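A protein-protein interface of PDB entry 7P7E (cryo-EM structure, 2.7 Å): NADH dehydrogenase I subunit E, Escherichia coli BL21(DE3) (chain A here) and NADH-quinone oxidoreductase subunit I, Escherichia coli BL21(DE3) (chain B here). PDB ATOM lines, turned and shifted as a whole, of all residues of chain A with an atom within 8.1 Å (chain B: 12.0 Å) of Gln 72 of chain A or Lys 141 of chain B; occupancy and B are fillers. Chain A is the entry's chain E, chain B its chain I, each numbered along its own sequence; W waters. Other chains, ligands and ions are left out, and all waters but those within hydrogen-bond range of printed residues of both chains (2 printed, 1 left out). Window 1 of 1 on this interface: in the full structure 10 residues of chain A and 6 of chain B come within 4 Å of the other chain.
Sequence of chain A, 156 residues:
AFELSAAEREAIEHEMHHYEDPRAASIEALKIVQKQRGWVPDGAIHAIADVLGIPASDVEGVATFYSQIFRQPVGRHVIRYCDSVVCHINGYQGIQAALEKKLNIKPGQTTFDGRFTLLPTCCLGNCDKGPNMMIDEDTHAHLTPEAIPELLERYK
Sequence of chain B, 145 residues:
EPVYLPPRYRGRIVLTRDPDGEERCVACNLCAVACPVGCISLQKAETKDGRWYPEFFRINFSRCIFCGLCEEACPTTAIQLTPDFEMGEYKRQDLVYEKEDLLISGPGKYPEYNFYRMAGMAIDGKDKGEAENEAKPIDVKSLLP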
ATOM      1  N   GLN A  34      33.032  27.415   9.562  1.00  0.00           N
ATOM      2  CA  GLN A  34      31.640  27.723   9.252  1.00  0.00           C
ATOM      3  C   GLN A  34      31.163  28.971   9.988  1.00  0.00           C
ATOM      4  O   GLN A  34      30.444  29.796   9.417  1.00  0.00           O
ATOM      5  CB  GLN A  34      30.763  26.518   9.594  1.00  0.00           C
ATOM      6  CG  GLN A  34      29.276  26.796   9.605  1.00  0.00           C
ATOM      7  CD  GLN A  34      28.463  25.589   9.206  1.00  0.00           C
ATOM      8  OE1 GLN A  34      28.610  25.065   8.106  1.00  0.00           O
ATOM      9  NE2 GLN A  34      27.598  25.137  10.105  1.00  0.00           N
ATOM     10  N   ARG A  37      32.846  32.011   8.154  1.00  0.00           N
ATOM     11  CA  ARG A  37      32.511  32.277   6.761  1.00  0.00           C
ATOM     12  C   ARG A  37      31.086  31.915   6.362  1.00  0.00           C
ATOM     13  O   ARG A  37      30.729  32.099   5.193  1.00  0.00           O
ATOM     14  CB  ARG A  37      33.488  31.543   5.831  1.00  0.00           C
ATOM     15  CG  ARG A  37      34.897  31.435   6.374  1.00  0.00           C
ATOM     16  CD  ARG A  37      35.930  31.587   5.277  1.00  0.00           C
ATOM     17  NE  ARG A  37      37.260  31.813   5.825  1.00  0.00           N
ATOM     18  CZ  ARG A  37      38.299  32.241   5.122  1.00  0.00           C
ATOM     19  NH1 ARG A  37      38.198  32.501   3.829  1.00  0.00           N
ATOM     20  NH2 ARG A  37      39.470  32.407   5.729  1.00  0.00           N
ATOM     21  N   GLY A  38      30.263  31.419   7.277  1.00  0.00           N
ATOM     22  CA  GLY A  38      28.904  31.006   6.954  1.00  0.00           C
ATOM     23  C   GLY A  38      28.787  29.540   6.585  1.00  0.00           C
ATOM     24  O   GLY A  38      27.797  28.889   6.921  1.00  0.00           O
ATOM     25  N   TRP A  39      29.798  29.007   5.906  1.00  0.00           N
ATOM     26  CA  TRP A  39      29.808  27.623   5.455  1.00  0.00           C
ATOM     27  C   TRP A  39      31.260  27.206   5.254  1.00  0.00           C
ATOM     28  O   TRP A  39      32.188  27.967   5.539  1.00  0.00           O
ATOM     29  CB  TRP A  39      28.975  27.447   4.181  1.00  0.00           C
ATOM     30  CG  TRP A  39      29.508  28.178   2.984  1.00  0.00           C
ATOM     31  CD1 TRP A  39      29.630  29.528   2.832  1.00  0.00           C
ATOM     32  CD2 TRP A  39      29.977  27.595   1.765  1.00  0.00           C
ATOM     33  NE1 TRP A  39      30.154  29.820   1.600  1.00  0.00           N
ATOM     34  CE2 TRP A  39      30.375  28.651   0.923  1.00  0.00           C
ATOM     35  CE3 TRP A  39      30.101  26.281   1.303  1.00  0.00           C
ATOM     36  CZ2 TRP A  39      30.888  28.434  -0.351  1.00  0.00           C
ATOM     37  CZ3 TRP A  39      30.610  26.071   0.038  1.00  0.00           C
ATOM     38  CH2 TRP A  39      30.998  27.141  -0.774  1.00  0.00           C
ATOM     39  N   VAL A  40      31.453  25.988   4.758  1.00  0.00           N
ATOM     40  CA  VAL A  40      32.776  25.398   4.595  1.00  0.00           C
ATOM     41  C   VAL A  40      33.009  25.156   3.104  1.00  0.00           C
ATOM     42  O   VAL A  40      32.420  24.228   2.531  1.00  0.00           O
ATOM     43  CB  VAL A  40      32.914  24.097   5.396  1.00  0.00           C
ATOM     44  CG1 VAL A  40      34.300  23.517   5.220  1.00  0.00           C
ATOM     45  CG2 VAL A  40      32.620  24.341   6.866  1.00  0.00           C
ATOM     46  N   PRO A  41      33.854  25.951   2.436  1.00  0.00           N
ATOM     47  CA  PRO A  41      34.206  25.649   1.040  1.00  0.00           C
ATOM     48  C   PRO A  41      35.217  24.514   0.909  1.00  0.00           C
ATOM     49  O   PRO A  41      35.645  23.939   1.913  1.00  0.00           O
ATOM     50  CB  PRO A  41      34.777  26.977   0.527  1.00  0.00           C
ATOM     51  CG  PRO A  41      35.234  27.697   1.741  1.00  0.00           C
ATOM     52  CD  PRO A  41      34.353  27.265   2.873  1.00  0.00           C
ATOM     53  N   ASP A  42      35.598  24.181  -0.328  1.00  0.00           N
ATOM     54  CA  ASP A  42      36.458  23.023  -0.573  1.00  0.00           C
ATOM     55  C   ASP A  42      37.899  23.292  -0.147  1.00  0.00           C
ATOM     56  O   ASP A  42      38.576  22.409   0.409  1.00  0.00           O
ATOM     57  CB  ASP A  42      36.402  22.653  -2.055  1.00  0.00           C
ATOM     58  CG  ASP A  42      34.986  22.657  -2.605  1.00  0.00           C
ATOM     59  OD1 ASP A  42      34.045  22.355  -1.844  1.00  0.00           O
ATOM     60  OD2 ASP A  42      34.814  22.968  -3.801  1.00  0.00           O
ATOM     61  N   ILE A  45      38.288  22.546   3.352  1.00  0.00           N
ATOM     62  CA  ILE A  45      38.517  21.125   3.615  1.00  0.00           C
ATOM     63  C   ILE A  45      39.999  20.799   3.492  1.00  0.00           C
ATOM     64  O   ILE A  45      40.592  20.165   4.377  1.00  0.00           O
ATOM     65  CB  ILE A  45      37.678  20.256   2.659  1.00  0.00           C
ATOM     66  CG1 ILE A  45      36.186  20.547   2.821  1.00  0.00           C
ATOM     67  CG2 ILE A  45      37.973  18.779   2.876  1.00  0.00           C
ATOM     68  CD1 ILE A  45      35.644  20.187   4.172  1.00  0.00           C
ATOM     69  N   GLU A  60      36.460  15.587   4.497  1.00  0.00           N
ATOM     70  CA  GLU A  60      35.259  15.701   3.677  1.00  0.00           C
ATOM     71  C   GLU A  60      34.192  14.698   4.101  1.00  0.00           C
ATOM     72  O   GLU A  60      32.997  15.013   4.079  1.00  0.00           O
ATOM     73  CB  GLU A  60      35.616  15.534   2.198  1.00  0.00           C
ATOM     74  CG  GLU A  60      34.433  15.620   1.237  1.00  0.00           C
ATOM     75  CD  GLU A  60      33.958  17.043   0.983  1.00  0.00           C
ATOM     76  OE1 GLU A  60      34.562  17.992   1.519  1.00  0.00           O
ATOM     77  OE2 GLU A  60      32.968  17.214   0.243  1.00  0.00           O
ATOM     78  N   ALA A  63      32.666  16.234   7.124  1.00  0.00           N
ATOM     79  CA  ALA A  63      31.871  17.413   6.788  1.00  0.00           C
ATOM     80  C   ALA A  63      30.554  17.039   6.122  1.00  0.00           C
ATOM     81  O   ALA A  63      29.523  17.671   6.376  1.00  0.00           O
ATOM     82  CB  ALA A  63      32.676  18.347   5.889  1.00  0.00           C
ATOM     83  N   THR A  64      30.563  16.017   5.270  1.00  0.00           N
ATOM     84  CA  THR A  64      29.338  15.581   4.617  1.00  0.00           C
ATOM     85  C   THR A  64      28.527  14.606   5.460  1.00  0.00           C
ATOM     86  O   THR A  64      27.367  14.351   5.126  1.00  0.00           O
ATOM     87  CB  THR A  64      29.661  14.942   3.266  1.00  0.00           C
ATOM     88  OG1 THR A  64      30.637  13.911   3.447  1.00  0.00           O
ATOM     89  CG2 THR A  64      30.203  15.982   2.297  1.00  0.00           C
ATOM     90  N   PHE A  65      29.098  14.046   6.531  1.00  0.00           N
ATOM     91  CA  PHE A  65      28.292  13.217   7.421  1.00  0.00           C
ATOM     92  C   PHE A  65      27.348  14.061   8.270  1.00  0.00           C
ATOM     93  O   PHE A  65      26.168  13.725   8.413  1.00  0.00           O
ATOM     94  CB  PHE A  65      29.189  12.364   8.316  1.00  0.00           C
ATOM     95  CG  PHE A  65      28.433  11.382   9.165  1.00  0.00           C
ATOM     96  CD1 PHE A  65      28.031  10.164   8.643  1.00  0.00           C
ATOM     97  CD2 PHE A  65      28.119  11.675  10.483  1.00  0.00           C
ATOM     98  CE1 PHE A  65      27.335   9.260   9.416  1.00  0.00           C
ATOM     99  CE2 PHE A  65      27.419  10.777  11.258  1.00  0.00           C
ATOM    100  CZ  PHE A  65      27.028   9.566  10.725  1.00  0.00           C
ATOM    101  N   SER A  67      24.995  17.116   9.469  1.00  0.00           N
ATOM    102  CA  SER A  67      24.073  17.977   8.736  1.00  0.00           C
ATOM    103  C   SER A  67      24.308  19.453   9.028  1.00  0.00           C
ATOM    104  O   SER A  67      24.003  20.300   8.182  1.00  0.00           O
ATOM    105  CB  SER A  67      22.632  17.595   9.067  1.00  0.00           C
ATOM    106  OG  SER A  67      22.362  17.782  10.443  1.00  0.00           O
ATOM    107  N   ILE A  69      27.152  20.990   9.397  1.00  0.00           N
ATOM    108  CA  ILE A  69      28.314  21.512   8.693  1.00  0.00           C
ATOM    109  C   ILE A  69      27.914  21.679   7.236  1.00  0.00           C
ATOM    110  O   ILE A  69      27.617  20.696   6.547  1.00  0.00           O
ATOM    111  CB  ILE A  69      29.530  20.585   8.844  1.00  0.00           C
ATOM    112  CG1 ILE A  69      30.041  20.626  10.283  1.00  0.00           C
ATOM    113  CG2 ILE A  69      30.632  20.992   7.884  1.00  0.00           C
ATOM    114  CD1 ILE A  69      30.906  19.449  10.656  1.00  0.00           C
ATOM    115  N   PHE A  70      27.890  22.922   6.770  1.00  0.00           N
ATOM    116  CA  PHE A  70      27.344  23.243   5.459  1.00  0.00           C
ATOM    117  C   PHE A  70      28.461  23.239   4.425  1.00  0.00           C
ATOM    118  O   PHE A  70      29.449  23.965   4.564  1.00  0.00           O
ATOM    119  CB  PHE A  70      26.641  24.598   5.489  1.00  0.00           C
ATOM    120  CG  PHE A  70      25.533  24.683   6.497  1.00  0.00           C
ATOM    121  CD1 PHE A  70      24.689  23.606   6.711  1.00  0.00           C
ATOM    122  CD2 PHE A  70      25.338  25.837   7.233  1.00  0.00           C
ATOM    123  CE1 PHE A  70      23.672  23.680   7.638  1.00  0.00           C
ATOM    124  CE2 PHE A  70      24.321  25.916   8.162  1.00  0.00           C
ATOM    125  CZ  PHE A  70      23.488  24.836   8.364  1.00  0.00           C
ATOM    126  N   ARG A  71      28.305  22.411   3.396  1.00  0.00           N
ATOM    127  CA  ARG A  71      29.249  22.346   2.292  1.00  0.00           C
ATOM    128  C   ARG A  71      28.722  23.044   1.045  1.00  0.00           C
ATOM    129  O   ARG A  71      29.323  22.925  -0.026  1.00  0.00           O
ATOM    130  CB  ARG A  71      29.595  20.889   1.988  1.00  0.00           C
ATOM    131  CG  ARG A  71      30.467  20.240   3.046  1.00  0.00           C
ATOM    132  CD  ARG A  71      31.868  20.803   3.006  1.00  0.00           C
ATOM    133  NE  ARG A  71      32.591  20.339   1.830  1.00  0.00           N
ATOM    134  CZ  ARG A  71      32.927  21.108   0.805  1.00  0.00           C
ATOM    135  NH1 ARG A  71      32.628  22.397   0.781  1.00  0.00           N
ATOM    136  NH2 ARG A  71      33.576  20.572  -0.224  1.00  0.00           N
ATOM    137  N   GLN A  72      27.611  23.761   1.163  1.00  0.00           N
ATOM    138  CA  GLN A  72      27.026  24.583   0.121  1.00  0.00           C
ATOM    139  C   GLN A  72      26.744  25.964   0.693  1.00  0.00           C
ATOM    140  O   GLN A  72      26.505  26.095   1.897  1.00  0.00           O
ATOM    141  CB  GLN A  72      25.728  23.961  -0.414  1.00  0.00           C
ATOM    142  CG  GLN A  72      25.946  22.938  -1.510  1.00  0.00           C
ATOM    143  CD  GLN A  72      24.677  22.208  -1.883  1.00  0.00           C
ATOM    144  OE1 GLN A  72      23.582  22.591  -1.473  1.00  0.00           O
ATOM    145  NE2 GLN A  72      24.815  21.144  -2.665  1.00  0.00           N
ATOM    146  N   PRO A  73      26.801  27.012  -0.132  1.00  0.00           N
ATOM    147  CA  PRO A  73      26.581  28.367   0.390  1.00  0.00           C
ATOM    148  C   PRO A  73      25.159  28.568   0.892  1.00  0.00           C
ATOM    149  O   PRO A  73      24.188  28.146   0.261  1.00  0.00           O
ATOM    150  CB  PRO A  73      26.879  29.268  -0.815  1.00  0.00           C
ATOM    151  CG  PRO A  73      26.777  28.380  -2.001  1.00  0.00           C
ATOM    152  CD  PRO A  73      27.226  27.035  -1.541  1.00  0.00           C
ATOM    153  N   VAL A  74      25.052  29.222   2.046  1.00  0.00           N
ATOM    154  CA  VAL A  74      23.766  29.487   2.678  1.00  0.00           C
ATOM    155  C   VAL A  74      23.536  30.990   2.713  1.00  0.00           C
ATOM    156  O   VAL A  74      24.401  31.772   2.304  1.00  0.00           O
ATOM    157  CB  VAL A  74      23.704  28.887   4.094  1.00  0.00           C
ATOM    158  CG1 VAL A  74      23.793  27.374   4.035  1.00  0.00           C
ATOM    159  CG2 VAL A  74      24.815  29.453   4.960  1.00  0.00           C
ATOM    160  N   GLY A  75      22.370  31.404   3.199  1.00  0.00           N
ATOM    161  CA  GLY A  75      22.051  32.807   3.328  1.00  0.00           C
ATOM    162  C   GLY A  75      22.659  33.413   4.577  1.00  0.00           C
ATOM    163  O   GLY A  75      23.466  32.803   5.280  1.00  0.00           O
ATOM    164  N   GLY A 108      15.293  23.934   2.029  1.00  0.00           N
ATOM    165  CA  GLY A 108      16.573  23.593   1.453  1.00  0.00           C
ATOM    166  C   GLY A 108      17.119  24.597   0.462  1.00  0.00           C
ATOM    167  O   GLY A 108      18.225  24.392  -0.049  1.00  0.00           O
ATOM    168  N   GLN A 109      16.387  25.668   0.174  1.00  0.00           N
ATOM    169  CA  GLN A 109      16.838  26.702  -0.744  1.00  0.00           C
ATOM    170  C   GLN A 109      17.145  27.988   0.010  1.00  0.00           C
ATOM    171  O   GLN A 109      16.900  28.116   1.212  1.00  0.00           O
ATOM    172  CB  GLN A 109      15.796  26.978  -1.833  1.00  0.00           C
ATOM    173  CG  GLN A 109      15.325  25.760  -2.591  1.00  0.00           C
ATOM    174  CD  GLN A 109      14.280  26.107  -3.630  1.00  0.00           C
ATOM    175  OE1 GLN A 109      13.328  26.833  -3.351  1.00  0.00           O
ATOM    176  NE2 GLN A 109      14.455  25.589  -4.839  1.00  0.00           N
ATOM    177  N   THR A 110      17.686  28.949  -0.730  1.00  0.00           N
ATOM    178  CA  THR A 110      18.042  30.260  -0.213  1.00  0.00           C
ATOM    179  C   THR A 110      17.261  31.308  -0.996  1.00  0.00           C
ATOM    180  O   THR A 110      17.018  31.139  -2.195  1.00  0.00           O
ATOM    181  CB  THR A 110      19.559  30.500  -0.337  1.00  0.00           C
ATOM    182  OG1 THR A 110      20.261  29.394   0.241  1.00  0.00           O
ATOM    183  CG2 THR A 110      19.985  31.769   0.387  1.00  0.00           C
ATOM    184  N   THR A 117      17.873  31.251   4.563  1.00  0.00           N
ATOM    185  CA  THR A 117      17.854  29.896   4.028  1.00  0.00           C
ATOM    186  C   THR A 117      17.023  29.021   4.955  1.00  0.00           C
ATOM    187  O   THR A 117      17.226  29.029   6.172  1.00  0.00           O
ATOM    188  CB  THR A 117      19.273  29.330   3.847  1.00  0.00           C
ATOM    189  OG1 THR A 117      19.209  27.913   3.648  1.00  0.00           O
ATOM    190  CG2 THR A 117      20.154  29.646   5.037  1.00  0.00           C
ATOM    191  N   LYS B 136      16.356  12.102  -9.050  1.00  0.00           N
ATOM    192  CA  LYS B 136      17.492  12.948  -9.372  1.00  0.00           C
ATOM    193  C   LYS B 136      18.637  12.678  -8.399  1.00  0.00           C
ATOM    194  O   LYS B 136      18.404  12.352  -7.233  1.00  0.00           O
ATOM    195  CB  LYS B 136      17.098  14.421  -9.312  1.00  0.00           C
ATOM    196  CG  LYS B 136      16.076  14.834 -10.350  1.00  0.00           C
ATOM    197  CD  LYS B 136      16.646  14.741 -11.753  1.00  0.00           C
ATOM    198  CE  LYS B 136      15.707  15.375 -12.765  1.00  0.00           C
ATOM    199  NZ  LYS B 136      14.969  16.531 -12.188  1.00  0.00           N
ATOM    200  N   PRO B 137      19.883  12.775  -8.862  1.00  0.00           N
ATOM    201  CA  PRO B 137      21.017  12.579  -7.953  1.00  0.00           C
ATOM    202  C   PRO B 137      21.095  13.686  -6.914  1.00  0.00           C
ATOM    203  O   PRO B 137      20.917  14.867  -7.220  1.00  0.00           O
ATOM    204  CB  PRO B 137      22.234  12.594  -8.884  1.00  0.00           C
ATOM    205  CG  PRO B 137      21.770  13.261 -10.121  1.00  0.00           C
ATOM    206  CD  PRO B 137      20.318  12.951 -10.257  1.00  0.00           C
ATOM    207  N   ILE B 138      21.357  13.287  -5.675  1.00  0.00           N
ATOM    208  CA  ILE B 138      21.480  14.206  -4.551  1.00  0.00           C
ATOM    209  C   ILE B 138      22.947  14.259  -4.161  1.00  0.00           C
ATOM    210  O   ILE B 138      23.537  13.234  -3.800  1.00  0.00           O
ATOM    211  CB  ILE B 138      20.608  13.771  -3.364  1.00  0.00           C
ATOM    212  CG1 ILE B 138      19.136  13.742  -3.769  1.00  0.00           C
ATOM    213  CG2 ILE B 138      20.820  14.697  -2.183  1.00  0.00           C
ATOM    214  CD1 ILE B 138      18.250  13.031  -2.784  1.00  0.00           C
ATOM    215  N   ASP B 139      23.537  15.447  -4.247  1.00  0.00           N
ATOM    216  CA  ASP B 139      24.922  15.626  -3.846  1.00  0.00           C
ATOM    217  C   ASP B 139      25.060  15.446  -2.340  1.00  0.00           C
ATOM    218  O   ASP B 139      24.151  15.761  -1.569  1.00  0.00           O
ATOM    219  CB  ASP B 139      25.423  17.010  -4.257  1.00  0.00           C
ATOM    220  CG  ASP B 139      26.905  17.024  -4.571  1.00  0.00           C
ATOM    221  OD1 ASP B 139      27.278  16.667  -5.708  1.00  0.00           O
ATOM    222  OD2 ASP B 139      27.701  17.392  -3.684  1.00  0.00           O
ATOM    223  N   VAL B 140      26.215  14.920  -1.923  1.00  0.00           N
ATOM    224  CA  VAL B 140      26.471  14.728  -0.501  1.00  0.00           C
ATOM    225  C   VAL B 140      26.702  16.051   0.210  1.00  0.00           C
ATOM    226  O   VAL B 140      26.663  16.105   1.443  1.00  0.00           O
ATOM    227  CB  VAL B 140      27.669  13.784  -0.288  1.00  0.00           C
ATOM    228  CG1 VAL B 140      27.316  12.390  -0.749  1.00  0.00           C
ATOM    229  CG2 VAL B 140      28.890  14.300  -1.029  1.00  0.00           C
ATOM    230  N   LYS B 141      26.939  17.123  -0.539  1.00  0.00           N
ATOM    231  CA  LYS B 141      27.130  18.454   0.013  1.00  0.00           C
ATOM    232  C   LYS B 141      25.824  19.212   0.200  1.00  0.00           C
ATOM    233  O   LYS B 141      25.858  20.385   0.580  1.00  0.00           O
ATOM    234  CB  LYS B 141      28.068  19.256  -0.890  1.00  0.00           C
ATOM    235  CG  LYS B 141      29.422  18.602  -1.093  1.00  0.00           C
ATOM    236  CD  LYS B 141      30.449  19.598  -1.592  1.00  0.00           C
ATOM    237  CE  LYS B 141      30.584  19.538  -3.102  1.00  0.00           C
ATOM    238  NZ  LYS B 141      29.547  20.358  -3.783  1.00  0.00           N
ATOM    239  N   SER B 142      24.684  18.574  -0.057  1.00  0.00           N
ATOM    240  CA  SER B 142      23.394  19.242   0.051  1.00  0.00           C
ATOM    241  C   SER B 142      23.062  19.564   1.504  1.00  0.00           C
ATOM    242  O   SER B 142      23.435  18.840   2.429  1.00  0.00           O
ATOM    243  CB  SER B 142      22.292  18.374  -0.552  1.00  0.00           C
ATOM    244  OG  SER B 142      21.854  17.392   0.369  1.00  0.00           O
ATOM    245  N   LEU B 143      22.349  20.675   1.693  1.00  0.00           N
ATOM    246  CA  LEU B 143      22.026  21.157   3.029  1.00  0.00           C
ATOM    247  C   LEU B 143      20.910  20.365   3.694  1.00  0.00           C
ATOM    248  O   LEU B 143      20.786  20.414   4.923  1.00  0.00           O
ATOM    249  CB  LEU B 143      21.634  22.632   2.968  1.00  0.00           C
ATOM    250  CG  LEU B 143      22.580  23.539   2.185  1.00  0.00           C
ATOM    251  CD1 LEU B 143      21.930  24.885   1.934  1.00  0.00           C
ATOM    252  CD2 LEU B 143      23.894  23.702   2.926  1.00  0.00           C
ATOM    253  N   LEU B 144      20.099  19.654   2.923  1.00  0.00           N
ATOM    254  CA  LEU B 144      19.015  18.881   3.508  1.00  0.00           C
ATOM    255  C   LEU B 144      19.571  17.653   4.223  1.00  0.00           C
ATOM    256  O   LEU B 144      20.513  17.021   3.734  1.00  0.00           O
ATOM    257  CB  LEU B 144      18.020  18.454   2.432  1.00  0.00           C
ATOM    258  CG  LEU B 144      17.139  19.568   1.868  1.00  0.00           C
ATOM    259  CD1 LEU B 144      16.296  19.054   0.717  1.00  0.00           C
ATOM    260  CD2 LEU B 144      16.264  20.154   2.960  1.00  0.00           C
ATOM    261  N   PRO B 145      19.015  17.289   5.389  1.00  0.00           N
ATOM    262  CA  PRO B 145      19.472  16.113   6.137  1.00  0.00           C
ATOM    263  C   PRO B 145      19.122  14.803   5.435  1.00  0.00           C
ATOM    264  O   PRO B 145      18.158  14.772   4.671  1.00  0.00           O
ATOM    265  CB  PRO B 145      18.726  16.227   7.474  1.00  0.00           C
ATOM    266  CG  PRO B 145      18.199  17.626   7.523  1.00  0.00           C
ATOM    267  CD  PRO B 145      17.959  18.018   6.108  1.00  0.00           C
HETATM  268  O   HOH W   1      26.015  20.823   3.275  1.00  0.00           O
HETATM  269  O   HOH W   2      30.089  23.345  -2.403  1.00  0.00           O
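The side-chain amide nitrogen (NE2) of Gln 72 of chain A lies close to the backbone carbonyl oxygen (O) of Lys 141 of chain B (3.5 Å).
The side-chain hydroxyl (OG1) of Thr 64 of chain A lies within hydrogen-bond range of the backbone carbonyl oxygen (O) of Glu 60 of chain A (2.7 Å).
O of Val 40 of chain A sits at hydrogen-bond distance from NH1 of Arg 71 of chain A, at 2.5 Å.
The side-chain carboxylate (OD2) of Asp 139 of chain B lies within salt-bridge range of the side-chain amino group (NZ) of Lys 141 of chain B (3.5 Å).
O of Phe 70 of chain A sits at hydrogen-bond distance from N of Val 40 of chain A.
The guanidinium group of Arg 71 of chain A is in salt-bridge range of the side-chain carboxylate of Glu 60 of chain A (3.1 Å).
NH2 of Arg 71 of chain A is in salt-bridge range of OD1 of Asp 42 of chain A (2.5 Å).
Among the printed residues, pairs that only touch across the chains: Glu 60 of chain A with Lys 141 of chain B (3.9 Å), Thr 64 of chain A with Val 140 of chain B (3.6 Å), Phe 70 of chain A with Leu 143 of chain B (3.9 Å), Arg 71 of chain A with Lys 141 of chain B (3.5 Å), Gln 72 of chain A with Ser 142 of chain B (3.6 Å), Gln 72 of chain A with Leu 143 of chain B (3.7 Å), Val 74 of chain A with Leu 143 of chain B (3.8 Å) and Gly 108 of chain A with Leu 144 of chain B (3.8 Å).
No residue of chain B comes within 4 Å of Trp 39 of chain A.
No residue of chain B comes within 4 Å of Val 40 of chain A.
Printed residues of chain B within 4 Å of Glu 60 of chain A: Lys 141.
Arg 71 of chain A touches just one residue of chain B: Lys 141 (3.5 Å).
Of chain B, only Lys 141, Ser 142 and Leu 143 come within 4 Å of Gln 72 of chain A.
Val 74 of chain A touches just one residue of chain B: Leu 143.
Of the printed residues of chain B, Gly 108 of chain A touches Leu 144 (3.8 Å).
Lys 136 of chain B touches none of the printed residues of chain A.
Printed residues of chain A within 4 Å of Val 140 of chain B: Thr 64.
Printed residues of chain A within 4 Å of Lys 141 of chain B: Glu 60 (3.9 Å), Arg 71 (3.5 Å) and Gln 72 (3.3 Å).
Of the printed residues of chain A, Ser 142 of chain B touches Gln 72 (3.6 Å).
The nearest residue of chain B that does not touch Gln 72 of chain A is Asp 139 of chain B (4.5 Å).
The nearest residue of chain A that does not touch Lys 141 of chain B is Thr 64 of chain A (4.4 Å).
The nearest printed residue of chain A that does not touch Val 140 of chain B is Glu 60 of chain A (5.2 Å).
Hydrophobic or aromatic side chains of chain A that line the printed part of chain B: Phe 70 and Val 74.
Along chain A the printed residues that touch a printed residue of chain B span positions 60 to 108.
Hydrophobic or aromatic side chains of chain B within 4 Å of the printed part of chain A: Val 140, Leu 143 and Leu 144.
Among the printed residues, 9 pairs touch across the chains.
Among the printed residues, no Asp or Glu carboxylate lies within 4 Å of a Lys or Arg side-chain nitrogen of the other chain.
Water W2 bridges the backbone carbonyl oxygen of Arg 71 of chain A (2.5 Å) and the side-chain amino group of Lys 141 of chain B (3.3 Å).
Water W1 lies within hydrogen-bond range of O of Lys 141 of chain B (2.7 Å), N of Arg 71 of chain A (2.8 Å) and O of Ser 142 of chain B (3.4 Å).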
